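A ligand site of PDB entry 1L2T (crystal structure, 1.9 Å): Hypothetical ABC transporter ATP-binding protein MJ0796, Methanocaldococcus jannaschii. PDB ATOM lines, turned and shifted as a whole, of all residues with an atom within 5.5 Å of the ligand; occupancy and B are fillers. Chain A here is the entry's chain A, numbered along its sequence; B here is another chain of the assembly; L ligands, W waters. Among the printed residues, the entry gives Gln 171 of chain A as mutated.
Water W5 lies within hydrogen-bond range of OE1 of Gln 90 (2.7 Å), O1 of the ligand (2.7 Å), O of Ala 175 of chain B (2.7 Å) and NE2 of Gln 171 (2.8 Å). Water W4 lies within hydrogen-bond range of O of Gly 41 (2.7 Å) and O12 of the ligand (2.9 Å). Water W1 lies within hydrogen-bond range of a nitrogen (N4) of the ligand (3.0 Å), the side-chain amide nitrogen of Gln 145 of chain B (3.4 Å) and the side-chain sulfur of Met 13 (3.6 Å). Water W3 lies within hydrogen-bond range of the backbone NH of Gly 148 of chain B, an oxygen (O7) of the ligand and the side-chain hydroxyl of Ser 45. Water W7 bridges O of Asn 144 of chain B (3.1 Å) and N3 of the ligand (3.1 Å). Water W9 lies within hydrogen-bond range of the side-chain hydroxyl of Ser 45, the side-chain amide nitrogen of Gln 171, the side-chain amide nitrogen of Gln 90 and an oxygen (O1) of the ligand.
Merely in contact with the ligand: Tyr 11 (3.5 Å), Met 13 (3.8 Å), Ala 20 (3.5 Å), Gln 90 (3.9 Å), Phe 138 of chain B (3.2 Å), His 141 of chain B (3.6 Å), Gln 145 of chain B (3.3 Å) and Ala 175 of chain B (3.8 Å). Of the 29 residues printed, 20 come within 4 Å of the ligand.
N of Thr 46 is in hydrogen-bond range of O8 of the ligand (3.1 Å). An oxygen (O8) of the ligand sits at hydrogen-bond distance from the side-chain hydroxyl (OG1) of Thr 46 (2.5 Å). The side-chain hydroxyl (OG) of Ser 40 sits at hydrogen-bond distance from an oxygen (O2) of the ligand, at 2.6 Å. O4 of the ligand lies within hydrogen-bond range of N of Gly 43 (2.6 Å). The side-chain hydroxyl (OG) of Ser 147 of chain B lies within hydrogen-bond range of an oxygen (O2) of the ligand, at 2.6 Å. N of Lys 44 sits at hydrogen-bond distance from O4 of the ligand (2.6 Å). NZ of Lys 44 is in salt-bridge range of O3 of the ligand, 3.0 Å away. The backbone NH (N) of Gly 41 sits at hydrogen-bond distance from an oxygen (O6) of the ligand. The backbone carbonyl oxygen of Gly 41 is in hydrogen-bond range of an oxygen (O12) of the ligand. An oxygen (O13) of the ligand is in hydrogen-bond range of the side-chain amide oxygen (OE1) of Gln 150 of chain B (2.7 Å). NE2 of His 204 sits at hydrogen-bond distance from O3 of the ligand. The backbone NH (N) of Gly 149 of chain B is in hydrogen-bond range of an oxygen (O2) of the ligand. N of Ser 45 is in hydrogen-bond range of O5 of the ligand, 2.9 Å away. OG of Ser 45 is in hydrogen-bond range of O5 of the ligand, at 3.1 Å. N of Ser 42 lies within hydrogen-bond range of O4 of the ligand, 3.2 Å away. The backbone NH (N) of Gly 148 of chain B is in hydrogen-bond range of an oxygen (O1) of the ligand (3.3 Å).
NH2 of Arg 153 of chain B sits at hydrogen-bond distance from OG of Ser 40 (2.7 Å). N of Ser 147 of chain B lies within hydrogen-bond range of OE1 of Gln 150 of chain B, 2.9 Å away. O of Pro 39 lies within hydrogen-bond range of NZ of Lys 44 (3.1 Å). The side-chain amino group of Lys 44 is in hydrogen-bond range of the backbone carbonyl oxygen of Gly 38, 2.9 Å away. O of Gly 149 of chain B lies within hydrogen-bond range of NE of Arg 153 of chain B (3.1 Å). OG of Ser 42 is in hydrogen-bond range of O of Pro 39 (2.8 Å). SD of Met 13 lies within hydrogen-bond range of NE2 of Gln 145 of chain B (3.6 Å). The backbone NH (N) of Tyr 11 is in hydrogen-bond range of the backbone carbonyl oxygen (O) of Ile 18 (2.7 Å).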
ATOM      1  N   TYR A  11      -0.085 -11.236  -3.540  1.00  0.00           N
ATOM      2  CA  TYR A  11      -0.742 -12.479  -3.937  1.00  0.00           C
ATOM      3  C   TYR A  11       0.261 -13.579  -3.724  1.00  0.00           C
ATOM      4  O   TYR A  11       1.460 -13.391  -3.958  1.00  0.00           O
ATOM      5  CB  TYR A  11      -1.159 -12.433  -5.403  1.00  0.00           C
ATOM      6  CG  TYR A  11      -2.222 -11.418  -5.674  1.00  0.00           C
ATOM      7  CD1 TYR A  11      -1.912 -10.179  -6.272  1.00  0.00           C
ATOM      8  CD2 TYR A  11      -3.554 -11.676  -5.336  1.00  0.00           C
ATOM      9  CE1 TYR A  11      -2.910  -9.226  -6.525  1.00  0.00           C
ATOM     10  CE2 TYR A  11      -4.568 -10.737  -5.580  1.00  0.00           C
ATOM     11  CZ  TYR A  11      -4.241  -9.516  -6.177  1.00  0.00           C
ATOM     12  OH  TYR A  11      -5.239  -8.600  -6.466  1.00  0.00           O
ATOM     13  N   MET A  13       1.473 -16.942  -5.098  1.00  0.00           N
ATOM     14  CA  MET A  13       1.423 -17.845  -6.244  1.00  0.00           C
ATOM     15  C   MET A  13       2.357 -19.010  -5.956  1.00  0.00           C
ATOM     16  O   MET A  13       3.571 -18.929  -6.213  1.00  0.00           O
ATOM     17  CB  MET A  13       1.876 -17.137  -7.501  1.00  0.00           C
ATOM     18  CG  MET A  13       0.912 -16.104  -7.996  1.00  0.00           C
ATOM     19  SD  MET A  13      -0.581 -16.814  -8.646  1.00  0.00           S
ATOM     20  CE  MET A  13       0.005 -17.662 -10.143  1.00  0.00           C
ATOM     21  N   ILE A  18       3.873 -12.192  -4.724  1.00  0.00           N
ATOM     22  CA  ILE A  18       3.701 -11.190  -5.771  1.00  0.00           C
ATOM     23  C   ILE A  18       3.117  -9.892  -5.181  1.00  0.00           C
ATOM     24  O   ILE A  18       2.060  -9.901  -4.550  1.00  0.00           O
ATOM     25  CB  ILE A  18       2.728 -11.704  -6.840  1.00  0.00           C
ATOM     26  CG1 ILE A  18       3.284 -12.970  -7.483  1.00  0.00           C
ATOM     27  CG2 ILE A  18       2.472 -10.647  -7.882  1.00  0.00           C
ATOM     28  CD1 ILE A  18       2.481 -13.435  -8.666  1.00  0.00           C
ATOM     29  N   ALA A  20       1.336  -6.747  -6.040  1.00  0.00           N
ATOM     30  CA  ALA A  20       0.551  -6.031  -7.059  1.00  0.00           C
ATOM     31  C   ALA A  20       0.756  -4.525  -6.816  1.00  0.00           C
ATOM     32  O   ALA A  20       0.833  -3.726  -7.761  1.00  0.00           O
ATOM     33  CB  ALA A  20      -0.935  -6.408  -6.970  1.00  0.00           C
ATOM     34  N   GLY A  38       0.722   3.853 -16.458  1.00  0.00           N
ATOM     35  CA  GLY A  38       1.794   2.961 -16.097  1.00  0.00           C
ATOM     36  C   GLY A  38       1.748   1.736 -16.982  1.00  0.00           C
ATOM     37  O   GLY A  38       0.711   1.435 -17.586  1.00  0.00           O
ATOM     38  N   PRO A  39       2.870   1.001 -17.104  1.00  0.00           N
ATOM     39  CA  PRO A  39       2.941  -0.197 -17.943  1.00  0.00           C
ATOM     40  C   PRO A  39       1.882  -1.255 -17.611  1.00  0.00           C
ATOM     41  O   PRO A  39       1.373  -1.317 -16.495  1.00  0.00           O
ATOM     42  CB  PRO A  39       4.327  -0.734 -17.637  1.00  0.00           C
ATOM     43  CG  PRO A  39       5.109   0.506 -17.352  1.00  0.00           C
ATOM     44  CD  PRO A  39       4.168   1.287 -16.472  1.00  0.00           C
ATOM     45  N   SER A  40       1.562  -2.077 -18.591  1.00  0.00           N
ATOM     46  CA  SER A  40       0.618  -3.136 -18.388  1.00  0.00           C
ATOM     47  C   SER A  40       1.180  -3.939 -17.200  1.00  0.00           C
ATOM     48  O   SER A  40       2.377  -4.211 -17.149  1.00  0.00           O
ATOM     49  CB  SER A  40       0.561  -4.016 -19.634  1.00  0.00           C
ATOM     50  OG  SER A  40      -0.220  -5.165 -19.380  1.00  0.00           O
ATOM     51  N   GLY A  41       0.334  -4.211 -16.222  1.00  0.00           N
ATOM     52  CA  GLY A  41       0.763  -4.974 -15.058  1.00  0.00           C
ATOM     53  C   GLY A  41       1.376  -4.169 -13.918  1.00  0.00           C
ATOM     54  O   GLY A  41       1.679  -4.747 -12.860  1.00  0.00           O
ATOM     55  N   SER A  42       1.522  -2.847 -14.075  1.00  0.00           N
ATOM     56  CA  SER A  42       2.124  -2.000 -13.032  1.00  0.00           C
ATOM     57  C   SER A  42       1.331  -1.812 -11.738  1.00  0.00           C
ATOM     58  O   SER A  42       1.862  -1.276 -10.775  1.00  0.00           O
ATOM     59  CB  SER A  42       2.449  -0.612 -13.578  1.00  0.00           C
ATOM     60  OG  SER A  42       1.299   0.028 -14.084  1.00  0.00           O
ATOM     61  N   GLY A  43       0.056  -2.208 -11.743  1.00  0.00           N
ATOM     62  CA  GLY A  43      -0.769  -2.104 -10.560  1.00  0.00           C
ATOM     63  C   GLY A  43      -1.908  -1.105 -10.587  1.00  0.00           C
ATOM     64  O   GLY A  43      -2.540  -0.873  -9.542  1.00  0.00           O
ATOM     65  N   LYS A  44      -2.213  -0.554 -11.760  1.00  0.00           N
ATOM     66  CA  LYS A  44      -3.274   0.461 -11.868  1.00  0.00           C
ATOM     67  C   LYS A  44      -4.683   0.029 -11.417  1.00  0.00           C
ATOM     68  O   LYS A  44      -5.347   0.755 -10.660  1.00  0.00           O
ATOM     69  CB  LYS A  44      -3.309   1.015 -13.288  1.00  0.00           C
ATOM     70  CG  LYS A  44      -1.946   1.511 -13.826  1.00  0.00           C
ATOM     71  CD  LYS A  44      -2.068   2.060 -15.252  1.00  0.00           C
ATOM     72  CE  LYS A  44      -2.492   0.995 -16.255  1.00  0.00           C
ATOM     73  NZ  LYS A  44      -1.419  -0.054 -16.401  1.00  0.00           N
ATOM     74  N   SER A  45      -5.160  -1.115 -11.909  1.00  0.00           N
ATOM     75  CA  SER A  45      -6.485  -1.604 -11.523  1.00  0.00           C
ATOM     76  C   SER A  45      -6.536  -2.035 -10.072  1.00  0.00           C
ATOM     77  O   SER A  45      -7.543  -1.837  -9.386  1.00  0.00           O
ATOM     78  CB  SER A  45      -6.968  -2.746 -12.421  1.00  0.00           C
ATOM     79  OG  SER A  45      -7.163  -2.305 -13.758  1.00  0.00           O
ATOM     80  N   THR A  46      -5.463  -2.637  -9.577  1.00  0.00           N
ATOM     81  CA  THR A  46      -5.430  -3.045  -8.176  1.00  0.00           C
ATOM     82  C   THR A  46      -5.660  -1.786  -7.334  1.00  0.00           C
ATOM     83  O   THR A  46      -6.505  -1.772  -6.422  1.00  0.00           O
ATOM     84  CB  THR A  46      -4.093  -3.640  -7.818  1.00  0.00           C
ATOM     85  OG1 THR A  46      -3.804  -4.716  -8.717  1.00  0.00           O
ATOM     86  CG2 THR A  46      -4.139  -4.171  -6.384  1.00  0.00           C
ATOM     87  N   MET A  47      -4.963  -0.710  -7.702  1.00  0.00           N
ATOM     88  CA  MET A  47      -5.084   0.548  -6.997  1.00  0.00           C
ATOM     89  C   MET A  47      -6.520   1.075  -7.073  1.00  0.00           C
ATOM     90  O   MET A  47      -7.135   1.375  -6.050  1.00  0.00           O
ATOM     91  CB  MET A  47      -4.119   1.580  -7.576  1.00  0.00           C
ATOM     92  CG  MET A  47      -4.229   2.923  -6.875  1.00  0.00           C
ATOM     93  SD  MET A  47      -2.948   4.054  -7.363  1.00  0.00           S
ATOM     94  CE  MET A  47      -1.567   3.347  -6.566  1.00  0.00           C
ATOM     95  N   GLN A  90     -13.137  -1.919 -16.532  1.00  0.00           N
ATOM     96  CA  GLN A  90     -12.458  -2.100 -17.814  1.00  0.00           C
ATOM     97  C   GLN A  90     -13.149  -3.201 -18.621  1.00  0.00           C
ATOM     98  O   GLN A  90     -13.310  -3.089 -19.831  1.00  0.00           O
ATOM     99  CB  GLN A  90     -10.994  -2.488 -17.588  1.00  0.00           C
ATOM    100  CG  GLN A  90     -10.245  -2.726 -18.879  1.00  0.00           C
ATOM    101  CD  GLN A  90      -8.769  -3.017 -18.671  1.00  0.00           C
ATOM    102  OE1 GLN A  90      -7.987  -2.986 -19.626  1.00  0.00           O
ATOM    103  NE2 GLN A  90      -8.383  -3.256 -17.423  1.00  0.00           N
ATOM    104  N   GLN A 171      -9.962   2.851 -17.647  1.00  0.00           N
ATOM    105  CA  GLN A 171      -9.789   2.925 -19.097  1.00  0.00           C
ATOM    106  C   GLN A 171     -11.144   3.080 -19.803  1.00  0.00           C
ATOM    107  O   GLN A 171     -11.474   2.343 -20.741  1.00  0.00           O
ATOM    108  CB  GLN A 171      -9.046   1.693 -19.572  1.00  0.00           C
ATOM    109  CG  GLN A 171      -7.674   1.669 -18.979  1.00  0.00           C
ATOM    110  CD  GLN A 171      -6.802   0.670 -19.633  1.00  0.00           C
ATOM    111  OE1 GLN A 171      -6.767   0.574 -20.850  1.00  0.00           O
ATOM    112  NE2 GLN A 171      -6.060  -0.066 -18.834  1.00  0.00           N
ATOM    113  N   VAL A 202      -7.927   5.736 -14.921  1.00  0.00           N
ATOM    114  CA  VAL A 202      -6.762   4.901 -15.235  1.00  0.00           C
ATOM    115  C   VAL A 202      -6.815   4.840 -16.761  1.00  0.00           C
ATOM    116  O   VAL A 202      -7.868   4.605 -17.342  1.00  0.00           O
ATOM    117  CB  VAL A 202      -6.890   3.475 -14.657  1.00  0.00           C
ATOM    118  CG1 VAL A 202      -5.860   2.565 -15.289  1.00  0.00           C
ATOM    119  CG2 VAL A 202      -6.735   3.497 -13.159  1.00  0.00           C
ATOM    120  N   HIS A 204      -4.367   4.265 -20.695  1.00  0.00           N
ATOM    121  CA  HIS A 204      -3.123   4.013 -21.410  1.00  0.00           C
ATOM    122  C   HIS A 204      -3.018   5.045 -22.520  1.00  0.00           C
ATOM    123  O   HIS A 204      -2.063   5.033 -23.288  1.00  0.00           O
ATOM    124  CB  HIS A 204      -3.124   2.617 -22.021  1.00  0.00           C
ATOM    125  CG  HIS A 204      -2.734   1.545 -21.061  1.00  0.00           C
ATOM    126  ND1 HIS A 204      -1.609   1.620 -20.257  1.00  0.00           N
ATOM    127  CD2 HIS A 204      -3.297   0.343 -20.788  1.00  0.00           C
ATOM    128  CE1 HIS A 204      -1.499   0.517 -19.537  1.00  0.00           C
ATOM    129  NE2 HIS A 204      -2.513  -0.281 -19.848  1.00  0.00           N
ATOM    130  N   PHE B 138       4.369 -15.329 -16.030  1.00  0.00           N
ATOM    131  CA  PHE B 138       2.912 -15.238 -16.020  1.00  0.00           C
ATOM    132  C   PHE B 138       2.229 -16.439 -16.681  1.00  0.00           C
ATOM    133  O   PHE B 138       1.030 -16.615 -16.540  1.00  0.00           O
ATOM    134  CB  PHE B 138       2.459 -13.924 -16.656  1.00  0.00           C
ATOM    135  CG  PHE B 138       2.825 -12.731 -15.850  1.00  0.00           C
ATOM    136  CD1 PHE B 138       3.769 -11.823 -16.301  1.00  0.00           C
ATOM    137  CD2 PHE B 138       2.273 -12.546 -14.574  1.00  0.00           C
ATOM    138  CE1 PHE B 138       4.178 -10.754 -15.500  1.00  0.00           C
ATOM    139  CE2 PHE B 138       2.660 -11.481 -13.771  1.00  0.00           C
ATOM    140  CZ  PHE B 138       3.619 -10.581 -14.220  1.00  0.00           C
ATOM    141  N   HIS B 141      -0.355 -18.319 -14.536  1.00  0.00           N
ATOM    142  CA  HIS B 141      -1.519 -17.617 -14.002  1.00  0.00           C
ATOM    143  C   HIS B 141      -2.774 -17.931 -14.813  1.00  0.00           C
ATOM    144  O   HIS B 141      -2.707 -18.123 -16.040  1.00  0.00           O
ATOM    145  CB  HIS B 141      -1.336 -16.099 -14.108  1.00  0.00           C
ATOM    146  CG  HIS B 141      -0.308 -15.533 -13.201  1.00  0.00           C
ATOM    147  ND1 HIS B 141      -0.529 -14.379 -12.472  1.00  0.00           N
ATOM    148  CD2 HIS B 141       0.964 -15.902 -12.929  1.00  0.00           C
ATOM    149  CE1 HIS B 141       0.567 -14.053 -11.821  1.00  0.00           C
ATOM    150  NE2 HIS B 141       1.498 -14.960 -12.076  1.00  0.00           N
ATOM    151  N   ASN B 144      -8.071 -14.954 -14.521  1.00  0.00           N
ATOM    152  CA  ASN B 144      -8.467 -14.093 -13.398  1.00  0.00           C
ATOM    153  C   ASN B 144      -7.311 -13.665 -12.501  1.00  0.00           C
ATOM    154  O   ASN B 144      -7.503 -12.882 -11.573  1.00  0.00           O
ATOM    155  CB  ASN B 144      -9.603 -14.729 -12.567  1.00  0.00           C
ATOM    156  CG  ASN B 144      -9.137 -15.909 -11.690  1.00  0.00           C
ATOM    157  OD1 ASN B 144      -7.995 -16.361 -11.749  1.00  0.00           O
ATOM    158  ND2 ASN B 144     -10.043 -16.390 -10.844  1.00  0.00           N
ATOM    159  N   GLN B 145      -6.123 -14.185 -12.753  1.00  0.00           N
ATOM    160  CA  GLN B 145      -4.942 -13.808 -11.977  1.00  0.00           C
ATOM    161  C   GLN B 145      -4.039 -12.897 -12.814  1.00  0.00           C
ATOM    162  O   GLN B 145      -2.874 -12.660 -12.464  1.00  0.00           O
ATOM    163  CB  GLN B 145      -4.154 -15.041 -11.544  1.00  0.00           C
ATOM    164  CG  GLN B 145      -4.993 -16.006 -10.747  1.00  0.00           C
ATOM    165  CD  GLN B 145      -4.233 -17.250 -10.425  1.00  0.00           C
ATOM    166  OE1 GLN B 145      -3.734 -17.928 -11.315  1.00  0.00           O
ATOM    167  NE2 GLN B 145      -4.114 -17.543  -9.145  1.00  0.00           N
ATOM    168  N   LEU B 146      -4.578 -12.389 -13.916  1.00  0.00           N
ATOM    169  CA  LEU B 146      -3.819 -11.537 -14.818  1.00  0.00           C
ATOM    170  C   LEU B 146      -4.516 -10.189 -14.989  1.00  0.00           C
ATOM    171  O   LEU B 146      -5.734 -10.088 -14.797  1.00  0.00           O
ATOM    172  CB  LEU B 146      -3.684 -12.210 -16.189  1.00  0.00           C
ATOM    173  CG  LEU B 146      -2.833 -13.483 -16.286  1.00  0.00           C
ATOM    174  CD1 LEU B 146      -2.964 -14.103 -17.658  1.00  0.00           C
ATOM    175  CD2 LEU B 146      -1.399 -13.167 -15.993  1.00  0.00           C
ATOM    176  N   SER B 147      -3.725  -9.162 -15.322  1.00  0.00           N
ATOM    177  CA  SER B 147      -4.263  -7.814 -15.567  1.00  0.00           C
ATOM    178  C   SER B 147      -4.877  -7.793 -16.972  1.00  0.00           C
ATOM    179  O   SER B 147      -4.632  -8.697 -17.770  1.00  0.00           O
ATOM    180  CB  SER B 147      -3.133  -6.794 -15.520  1.00  0.00           C
ATOM    181  OG  SER B 147      -2.237  -6.983 -16.584  1.00  0.00           O
ATOM    182  N   GLY B 148      -5.651  -6.748 -17.289  1.00  0.00           N
ATOM    183  CA  GLY B 148      -6.253  -6.664 -18.607  1.00  0.00           C
ATOM    184  C   GLY B 148      -5.279  -6.753 -19.775  1.00  0.00           C
ATOM    185  O   GLY B 148      -5.545  -7.431 -20.761  1.00  0.00           O
ATOM    186  N   GLY B 149      -4.140  -6.070 -19.647  1.00  0.00           N
ATOM    187  CA  GLY B 149      -3.115  -6.073 -20.692  1.00  0.00           C
ATOM    188  C   GLY B 149      -2.407  -7.418 -20.761  1.00  0.00           C
ATOM    189  O   GLY B 149      -1.961  -7.813 -21.848  1.00  0.00           O
ATOM    190  N   GLN B 150      -2.237  -8.083 -19.625  1.00  0.00           N
ATOM    191  CA  GLN B 150      -1.597  -9.410 -19.618  1.00  0.00           C
ATOM    192  C   GLN B 150      -2.536 -10.390 -20.306  1.00  0.00           C
ATOM    193  O   GLN B 150      -2.102 -11.203 -21.124  1.00  0.00           O
ATOM    194  CB  GLN B 150      -1.270  -9.859 -18.186  1.00  0.00           C
ATOM    195  CG  GLN B 150      -0.192  -8.998 -17.561  1.00  0.00           C
ATOM    196  CD  GLN B 150       0.016  -9.251 -16.077  1.00  0.00           C
ATOM    197  OE1 GLN B 150      -0.901  -9.683 -15.387  1.00  0.00           O
ATOM    198  NE2 GLN B 150       1.194  -8.931 -15.570  1.00  0.00           N
ATOM    199  N   ARG B 153      -2.355 -10.035 -23.980  1.00  0.00           N
ATOM    200  CA  ARG B 153      -1.189 -10.691 -24.549  1.00  0.00           C
ATOM    201  C   ARG B 153      -1.402 -12.197 -24.647  1.00  0.00           C
ATOM    202  O   ARG B 153      -0.925 -12.831 -25.593  1.00  0.00           O
ATOM    203  CB  ARG B 153       0.058 -10.322 -23.767  1.00  0.00           C
ATOM    204  CG  ARG B 153       0.524  -8.934 -24.118  1.00  0.00           C
ATOM    205  CD  ARG B 153       1.631  -8.451 -23.237  1.00  0.00           C
ATOM    206  NE  ARG B 153       1.166  -7.921 -21.961  1.00  0.00           N
ATOM    207  CZ  ARG B 153       1.949  -7.740 -20.900  1.00  0.00           C
ATOM    208  NH1 ARG B 153       3.234  -8.069 -20.985  1.00  0.00           N
ATOM    209  NH2 ARG B 153       1.484  -7.178 -19.787  1.00  0.00           N
ATOM    210  N   ALA B 175      -5.768  -2.683 -24.458  1.00  0.00           N
ATOM    211  CA  ALA B 175      -5.516  -2.756 -23.020  1.00  0.00           C
ATOM    212  C   ALA B 175      -4.032  -2.689 -22.716  1.00  0.00           C
ATOM    213  O   ALA B 175      -3.608  -3.006 -21.598  1.00  0.00           O
ATOM    214  CB  ALA B 175      -6.091  -4.059 -22.473  1.00  0.00           C
HETATM  215  P1  LIG L   1      -3.002  -3.583 -17.295  1.00  0.00           P
HETATM  216  O1  LIG L   1      -4.479  -3.689 -17.148  1.00  0.00           O
HETATM  217  O2  LIG L   1      -2.305  -4.730 -17.929  1.00  0.00           O
HETATM  218  O3  LIG L   1      -2.691  -2.313 -17.976  1.00  0.00           O
HETATM  219  P2  LIG L   1      -2.672  -2.778 -14.496  1.00  0.00           P
HETATM  220  O4  LIG L   1      -1.638  -2.179 -13.744  1.00  0.00           O
HETATM  221  O5  LIG L   1      -4.063  -2.479 -14.183  1.00  0.00           O
HETATM  222  O6  LIG L   1      -2.247  -3.338 -15.912  1.00  0.00           O
HETATM  223  P3  LIG L   1      -3.279  -4.634 -12.324  1.00  0.00           P
HETATM  224  O7  LIG L   1      -4.330  -5.585 -12.546  1.00  0.00           O
HETATM  225  O8  LIG L   1      -3.102  -3.995 -11.027  1.00  0.00           O
HETATM  226  O9  LIG L   1      -2.445  -4.170 -13.595  1.00  0.00           O
HETATM  227  O10 LIG L   1      -2.492  -5.812 -12.146  1.00  0.00           O
HETATM  228  C1  LIG L   1      -1.491  -6.507 -11.972  1.00  0.00           C
HETATM  229  C2  LIG L   1      -0.355  -7.082 -11.281  1.00  0.00           C
HETATM  230  O11 LIG L   1      -0.827  -7.898 -10.166  1.00  0.00           O
HETATM  231  C3  LIG L   1       0.012  -7.890 -12.468  1.00  0.00           C
HETATM  232  O12 LIG L   1       1.371  -8.050 -12.712  1.00  0.00           O
HETATM  233  C4  LIG L   1      -0.800  -9.185 -12.232  1.00  0.00           C
HETATM  234  O13 LIG L   1      -0.205 -10.328 -12.814  1.00  0.00           O
HETATM  235  C5  LIG L   1      -1.008  -9.278 -10.691  1.00  0.00           C
HETATM  236  N1  LIG L   1      -2.267  -9.881 -10.206  1.00  0.00           N
HETATM  237  C6  LIG L   1      -3.574  -9.401 -10.209  1.00  0.00           C
HETATM  238  N2  LIG L   1      -4.430 -10.241  -9.681  1.00  0.00           N
HETATM  239  C7  LIG L   1      -3.632 -11.318  -9.321  1.00  0.00           C
HETATM  240  C8  LIG L   1      -3.935 -12.581  -8.681  1.00  0.00           C
HETATM  241  N3  LIG L   1      -5.166 -12.927  -8.313  1.00  0.00           N
HETATM  242  N4  LIG L   1      -2.896 -13.450  -8.463  1.00  0.00           N
HETATM  243  C9  LIG L   1      -1.646 -13.131  -8.831  1.00  0.00           C
HETATM  244  N5  LIG L   1      -1.240 -11.999  -9.419  1.00  0.00           N
HETATM  245  C10 LIG L   1      -2.326 -11.108  -9.643  1.00  0.00           C
HETATM  246  O   HOH W   1      -3.231 -15.610  -6.473  1.00  0.00           O
HETATM  247  O   HOH W   2      -6.535 -15.463  -7.353  1.00  0.00           O
HETATM  248  O   HOH W   3      -6.172  -5.174 -14.918  1.00  0.00           O
HETATM  249  O   HOH W   4       3.396  -6.463 -14.007  1.00  0.00           O
HETATM  250  O   HOH W   5      -5.326  -2.692 -19.494  1.00  0.00           O
HETATM  251  O   HOH W   6       2.418  -9.912 -10.902  1.00  0.00           O
HETATM  252  O   HOH W   7      -7.483 -10.976  -9.150  1.00  0.00           O
HETATM  253  O   HOH W   8      -5.873  -7.502 -11.316  1.00  0.00           O
HETATM  254  O   HOH W   9      -6.511  -1.295 -16.218  1.00  0.00           O
